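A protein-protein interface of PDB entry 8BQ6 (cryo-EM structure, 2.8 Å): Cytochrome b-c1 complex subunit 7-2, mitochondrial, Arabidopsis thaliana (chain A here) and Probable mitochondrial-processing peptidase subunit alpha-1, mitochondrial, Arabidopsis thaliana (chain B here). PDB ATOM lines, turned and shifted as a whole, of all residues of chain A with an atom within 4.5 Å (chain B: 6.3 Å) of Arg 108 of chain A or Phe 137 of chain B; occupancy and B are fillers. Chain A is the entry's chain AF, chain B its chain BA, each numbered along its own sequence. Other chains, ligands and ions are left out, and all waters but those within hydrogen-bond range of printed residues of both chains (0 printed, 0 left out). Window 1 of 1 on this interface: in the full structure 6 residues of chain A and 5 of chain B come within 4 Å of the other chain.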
ATOM      1  N   GLU A 104      14.633 -16.155  18.769  1.00  0.00           N
ATOM      2  CA  GLU A 104      14.242 -14.825  18.324  1.00  0.00           C
ATOM      3  C   GLU A 104      13.206 -14.898  17.213  1.00  0.00           C
ATOM      4  O   GLU A 104      12.351 -14.013  17.093  1.00  0.00           O
ATOM      5  CB  GLU A 104      15.472 -14.046  17.866  1.00  0.00           C
ATOM      6  CG  GLU A 104      16.409 -13.703  19.001  1.00  0.00           C
ATOM      7  CD  GLU A 104      17.677 -13.044  18.526  1.00  0.00           C
ATOM      8  OE1 GLU A 104      17.989 -13.146  17.321  1.00  0.00           O
ATOM      9  OE2 GLU A 104      18.356 -12.412  19.360  1.00  0.00           O
ATOM     10  N   ARG A 105      13.277 -15.938  16.380  1.00  0.00           N
ATOM     11  CA  ARG A 105      12.256 -16.127  15.356  1.00  0.00           C
ATOM     12  C   ARG A 105      10.904 -16.454  15.977  1.00  0.00           C
ATOM     13  O   ARG A 105       9.868 -15.977  15.502  1.00  0.00           O
ATOM     14  CB  ARG A 105      12.682 -17.225  14.385  1.00  0.00           C
ATOM     15  CG  ARG A 105      13.458 -16.703  13.198  1.00  0.00           C
ATOM     16  CD  ARG A 105      12.969 -17.310  11.891  1.00  0.00           C
ATOM     17  NE  ARG A 105      13.164 -18.753  11.827  1.00  0.00           N
ATOM     18  CZ  ARG A 105      12.221 -19.655  12.061  1.00  0.00           C
ATOM     19  NH1 ARG A 105      10.992 -19.301  12.399  1.00  0.00           N
ATOM     20  NH2 ARG A 105      12.520 -20.947  11.956  1.00  0.00           N
ATOM     21  N   ALA A 106      10.893 -17.266  17.035  1.00  0.00           N
ATOM     22  CA  ALA A 106       9.635 -17.593  17.699  1.00  0.00           C
ATOM     23  C   ALA A 106       9.034 -16.366  18.372  1.00  0.00           C
ATOM     24  O   ALA A 106       7.808 -16.231  18.454  1.00  0.00           O
ATOM     25  CB  ALA A 106       9.851 -18.712  18.716  1.00  0.00           C
ATOM     26  N   GLU A 107       9.884 -15.469  18.872  1.00  0.00           N
ATOM     27  CA  GLU A 107       9.396 -14.236  19.478  1.00  0.00           C
ATOM     28  C   GLU A 107       8.757 -13.324  18.438  1.00  0.00           C
ATOM     29  O   GLU A 107       7.755 -12.656  18.720  1.00  0.00           O
ATOM     30  CB  GLU A 107      10.540 -13.520  20.187  1.00  0.00           C
ATOM     31  CG  GLU A 107      10.108 -12.328  21.004  1.00  0.00           C
ATOM     32  CD  GLU A 107      11.286 -11.530  21.513  1.00  0.00           C
ATOM     33  OE1 GLU A 107      12.361 -11.586  20.881  1.00  0.00           O
ATOM     34  OE2 GLU A 107      11.142 -10.864  22.558  1.00  0.00           O
ATOM     35  N   ARG A 108       9.338 -13.260  17.239  1.00  0.00           N
ATOM     36  CA  ARG A 108       8.736 -12.463  16.177  1.00  0.00           C
ATOM     37  C   ARG A 108       7.388 -13.033  15.759  1.00  0.00           C
ATOM     38  O   ARG A 108       6.429 -12.284  15.542  1.00  0.00           O
ATOM     39  CB  ARG A 108       9.682 -12.385  14.980  1.00  0.00           C
ATOM     40  CG  ARG A 108      10.918 -11.569  15.259  1.00  0.00           C
ATOM     41  CD  ARG A 108      11.626 -11.156  13.990  1.00  0.00           C
ATOM     42  NE  ARG A 108      10.812 -10.265  13.174  1.00  0.00           N
ATOM     43  CZ  ARG A 108      11.052  -8.971  13.019  1.00  0.00           C
ATOM     44  NH1 ARG A 108      12.008  -8.360  13.697  1.00  0.00           N
ATOM     45  NH2 ARG A 108      10.305  -8.270  12.172  1.00  0.00           N
ATOM     46  N   GLU A 109       7.298 -14.361  15.647  1.00  0.00           N
ATOM     47  CA  GLU A 109       6.049 -15.004  15.247  1.00  0.00           C
ATOM     48  C   GLU A 109       4.953 -14.796  16.285  1.00  0.00           C
ATOM     49  O   GLU A 109       3.796 -14.542  15.932  1.00  0.00           O
ATOM     50  CB  GLU A 109       6.282 -16.497  15.018  1.00  0.00           C
ATOM     51  CG  GLU A 109       6.544 -16.890  13.573  1.00  0.00           C
ATOM     52  CD  GLU A 109       7.728 -17.833  13.433  1.00  0.00           C
ATOM     53  OE1 GLU A 109       7.869 -18.746  14.275  1.00  0.00           O
ATOM     54  OE2 GLU A 109       8.521 -17.659  12.484  1.00  0.00           O
ATOM     55  N   ALA A 110       5.296 -14.912  17.570  1.00  0.00           N
ATOM     56  CA  ALA A 110       4.308 -14.767  18.632  1.00  0.00           C
ATOM     57  C   ALA A 110       3.717 -13.367  18.695  1.00  0.00           C
ATOM     58  O   ALA A 110       2.633 -13.189  19.261  1.00  0.00           O
ATOM     59  CB  ALA A 110       4.937 -15.119  19.979  1.00  0.00           C
ATOM     60  N   LEU A 111       4.405 -12.373  18.138  1.00  0.00           N
ATOM     61  CA  LEU A 111       3.951 -10.992  18.157  1.00  0.00           C
ATOM     62  C   LEU A 111       3.476 -10.518  16.789  1.00  0.00           C
ATOM     63  O   LEU A 111       3.235  -9.322  16.606  1.00  0.00           O
ATOM     64  CB  LEU A 111       5.072 -10.087  18.670  1.00  0.00           C
ATOM     65  CG  LEU A 111       5.431 -10.204  20.155  1.00  0.00           C
ATOM     66  CD1 LEU A 111       6.323  -9.053  20.575  1.00  0.00           C
ATOM     67  CD2 LEU A 111       4.190 -10.252  21.023  1.00  0.00           C
ATOM     68  N   GLY A 112       3.344 -11.426  15.825  1.00  0.00           N
ATOM     69  CA  GLY A 112       2.812 -11.067  14.527  1.00  0.00           C
ATOM     70  C   GLY A 112       3.733 -10.246  13.661  1.00  0.00           C
ATOM     71  O   GLY A 112       3.272  -9.627  12.697  1.00  0.00           O
ATOM     72  N   ALA A 113       5.022 -10.212  13.974  1.00  0.00           N
ATOM     73  CA  ALA A 113       5.970  -9.466  13.170  1.00  0.00           C
ATOM     74  C   ALA A 113       6.321 -10.235  11.900  1.00  0.00           C
ATOM     75  O   ALA A 113       6.099 -11.444  11.791  1.00  0.00           O
ATOM     76  CB  ALA A 113       7.233  -9.173  13.973  1.00  0.00           C
ATOM     77  N   LEU A 114       6.863  -9.513  10.929  1.00  0.00           N
ATOM     78  CA  LEU A 114       7.309 -10.147   9.699  1.00  0.00           C
ATOM     79  C   LEU A 114       8.626 -10.884   9.937  1.00  0.00           C
ATOM     80  O   LEU A 114       9.419 -10.481  10.791  1.00  0.00           O
ATOM     81  CB  LEU A 114       7.482  -9.105   8.596  1.00  0.00           C
ATOM     82  CG  LEU A 114       6.210  -8.594   7.920  1.00  0.00           C
ATOM     83  CD1 LEU A 114       6.540  -7.993   6.570  1.00  0.00           C
ATOM     84  CD2 LEU A 114       5.209  -9.722   7.763  1.00  0.00           C
ATOM     85  N   LEU A 116      12.450 -11.961   9.569  1.00  0.00           N
ATOM     86  CA  LEU A 116      13.640 -11.200   9.205  1.00  0.00           C
ATOM     87  C   LEU A 116      14.299 -11.717   7.937  1.00  0.00           C
ATOM     88  O   LEU A 116      15.045 -10.974   7.291  1.00  0.00           O
ATOM     89  CB  LEU A 116      14.652 -11.226  10.347  1.00  0.00           C
ATOM     90  CG  LEU A 116      14.453 -10.209  11.468  1.00  0.00           C
ATOM     91  CD1 LEU A 116      15.597 -10.298  12.446  1.00  0.00           C
ATOM     92  CD2 LEU A 116      14.359  -8.814  10.887  1.00  0.00           C
ATOM     93  N   SER B 130      19.401  -4.045  21.938  1.00  0.00           N
ATOM     94  CA  SER B 130      19.210  -5.234  22.761  1.00  0.00           C
ATOM     95  C   SER B 130      19.906  -5.099  24.110  1.00  0.00           C
ATOM     96  O   SER B 130      21.050  -4.647  24.197  1.00  0.00           O
ATOM     97  CB  SER B 130      19.746  -6.468  22.037  1.00  0.00           C
ATOM     98  OG  SER B 130      18.924  -6.824  20.943  1.00  0.00           O
ATOM     99  N   ARG B 134      16.070  -8.189  27.376  1.00  0.00           N
ATOM    100  CA  ARG B 134      15.057  -8.111  26.334  1.00  0.00           C
ATOM    101  C   ARG B 134      15.721  -7.797  25.005  1.00  0.00           C
ATOM    102  O   ARG B 134      16.610  -6.944  24.930  1.00  0.00           O
ATOM    103  CB  ARG B 134      14.000  -7.048  26.645  1.00  0.00           C
ATOM    104  CG  ARG B 134      14.555  -5.840  27.345  1.00  0.00           C
ATOM    105  CD  ARG B 134      13.625  -4.657  27.260  1.00  0.00           C
ATOM    106  NE  ARG B 134      12.381  -4.870  27.985  1.00  0.00           N
ATOM    107  CZ  ARG B 134      12.199  -4.582  29.266  1.00  0.00           C
ATOM    108  NH1 ARG B 134      13.188  -4.127  30.021  1.00  0.00           N
ATOM    109  NH2 ARG B 134      10.998  -4.762  29.807  1.00  0.00           N
ATOM    110  N   THR B 135      15.268  -8.477  23.961  1.00  0.00           N
ATOM    111  CA  THR B 135      15.825  -8.252  22.643  1.00  0.00           C
ATOM    112  C   THR B 135      15.436  -6.872  22.129  1.00  0.00           C
ATOM    113  O   THR B 135      14.521  -6.217  22.637  1.00  0.00           O
ATOM    114  CB  THR B 135      15.352  -9.325  21.670  1.00  0.00           C
ATOM    115  OG1 THR B 135      13.924  -9.277  21.560  1.00  0.00           O
ATOM    116  CG2 THR B 135      15.761 -10.692  22.173  1.00  0.00           C
ATOM    117  N   HIS B 136      16.168  -6.428  21.111  1.00  0.00           N
ATOM    118  CA  HIS B 136      15.852  -5.159  20.474  1.00  0.00           C
ATOM    119  C   HIS B 136      14.433  -5.168  19.922  1.00  0.00           C
ATOM    120  O   HIS B 136      13.725  -4.157  19.988  1.00  0.00           O
ATOM    121  CB  HIS B 136      16.876  -4.881  19.377  1.00  0.00           C
ATOM    122  CG  HIS B 136      16.729  -3.544  18.728  1.00  0.00           C
ATOM    123  ND1 HIS B 136      17.176  -3.292  17.450  1.00  0.00           N
ATOM    124  CD2 HIS B 136      16.190  -2.386  19.175  1.00  0.00           C
ATOM    125  CE1 HIS B 136      16.918  -2.035  17.136  1.00  0.00           C
ATOM    126  NE2 HIS B 136      16.318  -1.464  18.165  1.00  0.00           N
ATOM    127  N   PHE B 137      13.992  -6.313  19.393  1.00  0.00           N
ATOM    128  CA  PHE B 137      12.636  -6.414  18.868  1.00  0.00           C
ATOM    129  C   PHE B 137      11.600  -6.215  19.966  1.00  0.00           C
ATOM    130  O   PHE B 137      10.618  -5.487  19.783  1.00  0.00           O
ATOM    131  CB  PHE B 137      12.430  -7.764  18.181  1.00  0.00           C
ATOM    132  CG  PHE B 137      10.993  -8.061  17.861  1.00  0.00           C
ATOM    133  CD1 PHE B 137      10.358  -7.417  16.814  1.00  0.00           C
ATOM    134  CD2 PHE B 137      10.274  -8.968  18.615  1.00  0.00           C
ATOM    135  CE1 PHE B 137       9.040  -7.683  16.519  1.00  0.00           C
ATOM    136  CE2 PHE B 137       8.957  -9.237  18.325  1.00  0.00           C
ATOM    137  CZ  PHE B 137       8.338  -8.593  17.278  1.00  0.00           C
ATOM    138  N   ARG B 138      11.797  -6.856  21.119  1.00  0.00           N
ATOM    139  CA  ARG B 138      10.831  -6.694  22.198  1.00  0.00           C
ATOM    140  C   ARG B 138      10.863  -5.284  22.773  1.00  0.00           C
ATOM    141  O   ARG B 138       9.823  -4.762  23.188  1.00  0.00           O
ATOM    142  CB  ARG B 138      11.079  -7.721  23.298  1.00  0.00           C
ATOM    143  CG  ARG B 138      10.145  -7.560  24.479  1.00  0.00           C
ATOM    144  CD  ARG B 138      10.510  -8.486  25.609  1.00  0.00           C
ATOM    145  NE  ARG B 138       9.978  -8.010  26.879  1.00  0.00           N
ATOM    146  CZ  ARG B 138       8.973  -8.578  27.528  1.00  0.00           C
ATOM    147  NH1 ARG B 138       8.367  -9.655  27.057  1.00  0.00           N
ATOM    148  NH2 ARG B 138       8.566  -8.054  28.679  1.00  0.00           N
ATOM    149  N   LEU B 139      12.040  -4.659  22.811  1.00  0.00           N
ATOM    150  CA  LEU B 139      12.146  -3.294  23.319  1.00  0.00           C
ATOM    151  C   LEU B 139      11.359  -2.321  22.449  1.00  0.00           C
ATOM    152  O   LEU B 139      10.604  -1.485  22.958  1.00  0.00           O
ATOM    153  CB  LEU B 139      13.614  -2.885  23.389  1.00  0.00           C
ATOM    154  CG  LEU B 139      13.950  -1.588  24.120  1.00  0.00           C
ATOM    155  CD1 LEU B 139      13.390  -1.622  25.519  1.00  0.00           C
ATOM    156  CD2 LEU B 139      15.443  -1.383  24.151  1.00  0.00           C
ATOM    157  N   VAL B 140      11.527  -2.417  21.128  1.00  0.00           N
ATOM    158  CA  VAL B 140      10.779  -1.559  20.214  1.00  0.00           C
ATOM    159  C   VAL B 140       9.283  -1.808  20.357  1.00  0.00           C
ATOM    160  O   VAL B 140       8.476  -0.870  20.331  1.00  0.00           O
ATOM    161  CB  VAL B 140      11.255  -1.785  18.767  1.00  0.00           C
ATOM    162  CG1 VAL B 140      10.320  -1.107  17.780  1.00  0.00           C
ATOM    163  CG2 VAL B 140      12.677  -1.281  18.591  1.00  0.00           C
ATOM    164  N   ARG B 141       8.892  -3.071  20.524  1.00  0.00           N
ATOM    165  CA  ARG B 141       7.475  -3.398  20.645  1.00  0.00           C
ATOM    166  C   ARG B 141       6.895  -2.897  21.962  1.00  0.00           C
ATOM    167  O   ARG B 141       5.704  -2.575  22.036  1.00  0.00           O
ATOM    168  CB  ARG B 141       7.272  -4.905  20.505  1.00  0.00           C
ATOM    169  CG  ARG B 141       7.289  -5.408  19.073  1.00  0.00           C
ATOM    170  CD  ARG B 141       6.411  -4.552  18.183  1.00  0.00           C
ATOM    171  NE  ARG B 141       6.541  -4.883  16.770  1.00  0.00           N
ATOM    172  CZ  ARG B 141       5.788  -5.772  16.136  1.00  0.00           C
ATOM    173  NH1 ARG B 141       4.854  -6.462  16.767  1.00  0.00           N
ATOM    174  NH2 ARG B 141       5.970  -5.964  14.832  1.00  0.00           N
ATOM    175  N   GLU B 142       7.712  -2.837  23.017  1.00  0.00           N
ATOM    176  CA  GLU B 142       7.227  -2.319  24.293  1.00  0.00           C
ATOM    177  C   GLU B 142       7.010  -0.812  24.235  1.00  0.00           C
ATOM    178  O   GLU B 142       6.033  -0.294  24.789  1.00  0.00           O
ATOM    179  CB  GLU B 142       8.205  -2.669  25.411  1.00  0.00           C
ATOM    180  CG  GLU B 142       8.090  -4.092  25.913  1.00  0.00           C
ATOM    181  CD  GLU B 142       9.328  -4.540  26.654  1.00  0.00           C
ATOM    182  OE1 GLU B 142      10.406  -3.967  26.400  1.00  0.00           O
ATOM    183  OE2 GLU B 142       9.228  -5.469  27.482  1.00  0.00           O
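Of chain B, only Phe 137 (3.7 Å) comes within 4 Å of Arg 108 of chain A. Phe 137 of chain B touches just these residues of chain A: Glu 107 (3.6 Å), Arg 108 (3.7 Å), Leu 111 (3.5 Å) and Ala 113 (3.5 Å). Printed residues of chain A within 4 Å of Arg 138 of chain B: Glu 107. Of the printed residues of chain B, Leu 111 of chain A touches Phe 137 and Arg 141. Of the printed residues of chain B, Glu 107 of chain A touches Thr 135 (2.9 Å), Phe 137 (3.6 Å) and Arg 138 (3.2 Å). Ser 130 of chain B touches none of the printed residues of chain A. Glu 142 of chain B touches none of the printed residues of chain A. The nearest printed residue of chain A that does not touch Phe 137 of chain B is Glu 104 of chain A (5.7 Å). The nearest printed residue of chain B that does not touch Ala 113 of chain A is Arg 138 of chain B (8.8 Å).
Hydrophobic or aromatic side chains of chain A within 4 Å of the printed part of chain B: Leu 111 and Ala 113. Printed residues of chain B that touch a printed residue of chain A: Thr 135, Phe 137, Arg 138 and Arg 141. Among the printed residues, no Asp or Glu carboxylate lies within 4 Å of a Lys or Arg side-chain nitrogen of the other chain.
Among the printed residues, pairs that only touch across the chains: Glu 107 of chain A with Phe 137 of chain B (3.6 Å), Glu 107 of chain A with Arg 138 of chain B (3.2 Å), Arg 108 of chain A with Phe 137 of chain B (3.7 Å), Leu 111 of chain A with Phe 137 of chain B (3.5 Å), Ala 113 of chain A with Phe 137 of chain B (3.5 Å) and Ala 113 of chain A with Arg 141 of chain B (3.6 Å).
The side-chain carboxylate of Glu 107 of chain A lies within hydrogen-bond range of the side-chain hydroxyl of Thr 135 of chain B. NH1 of Arg 141 of chain B lies within hydrogen-bond range of O of Leu 111 of chain A (3.3 Å).
NH2 of Arg 108 of chain A is in hydrogen-bond range of O of Leu 114 of chain A. O of Arg 108 of chain A lies within hydrogen-bond range of N of Ala 113 of chain A (3.0 Å). The guanidinium group (NE) of Arg 138 of chain B lies within salt-bridge range of the side-chain carboxylate (OE2) of Glu 142 of chain B. The backbone NH (N) of Arg 138 of chain B lies within hydrogen-bond range of the side-chain hydroxyl (OG1) of Thr 135 of chain B (3.3 Å).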
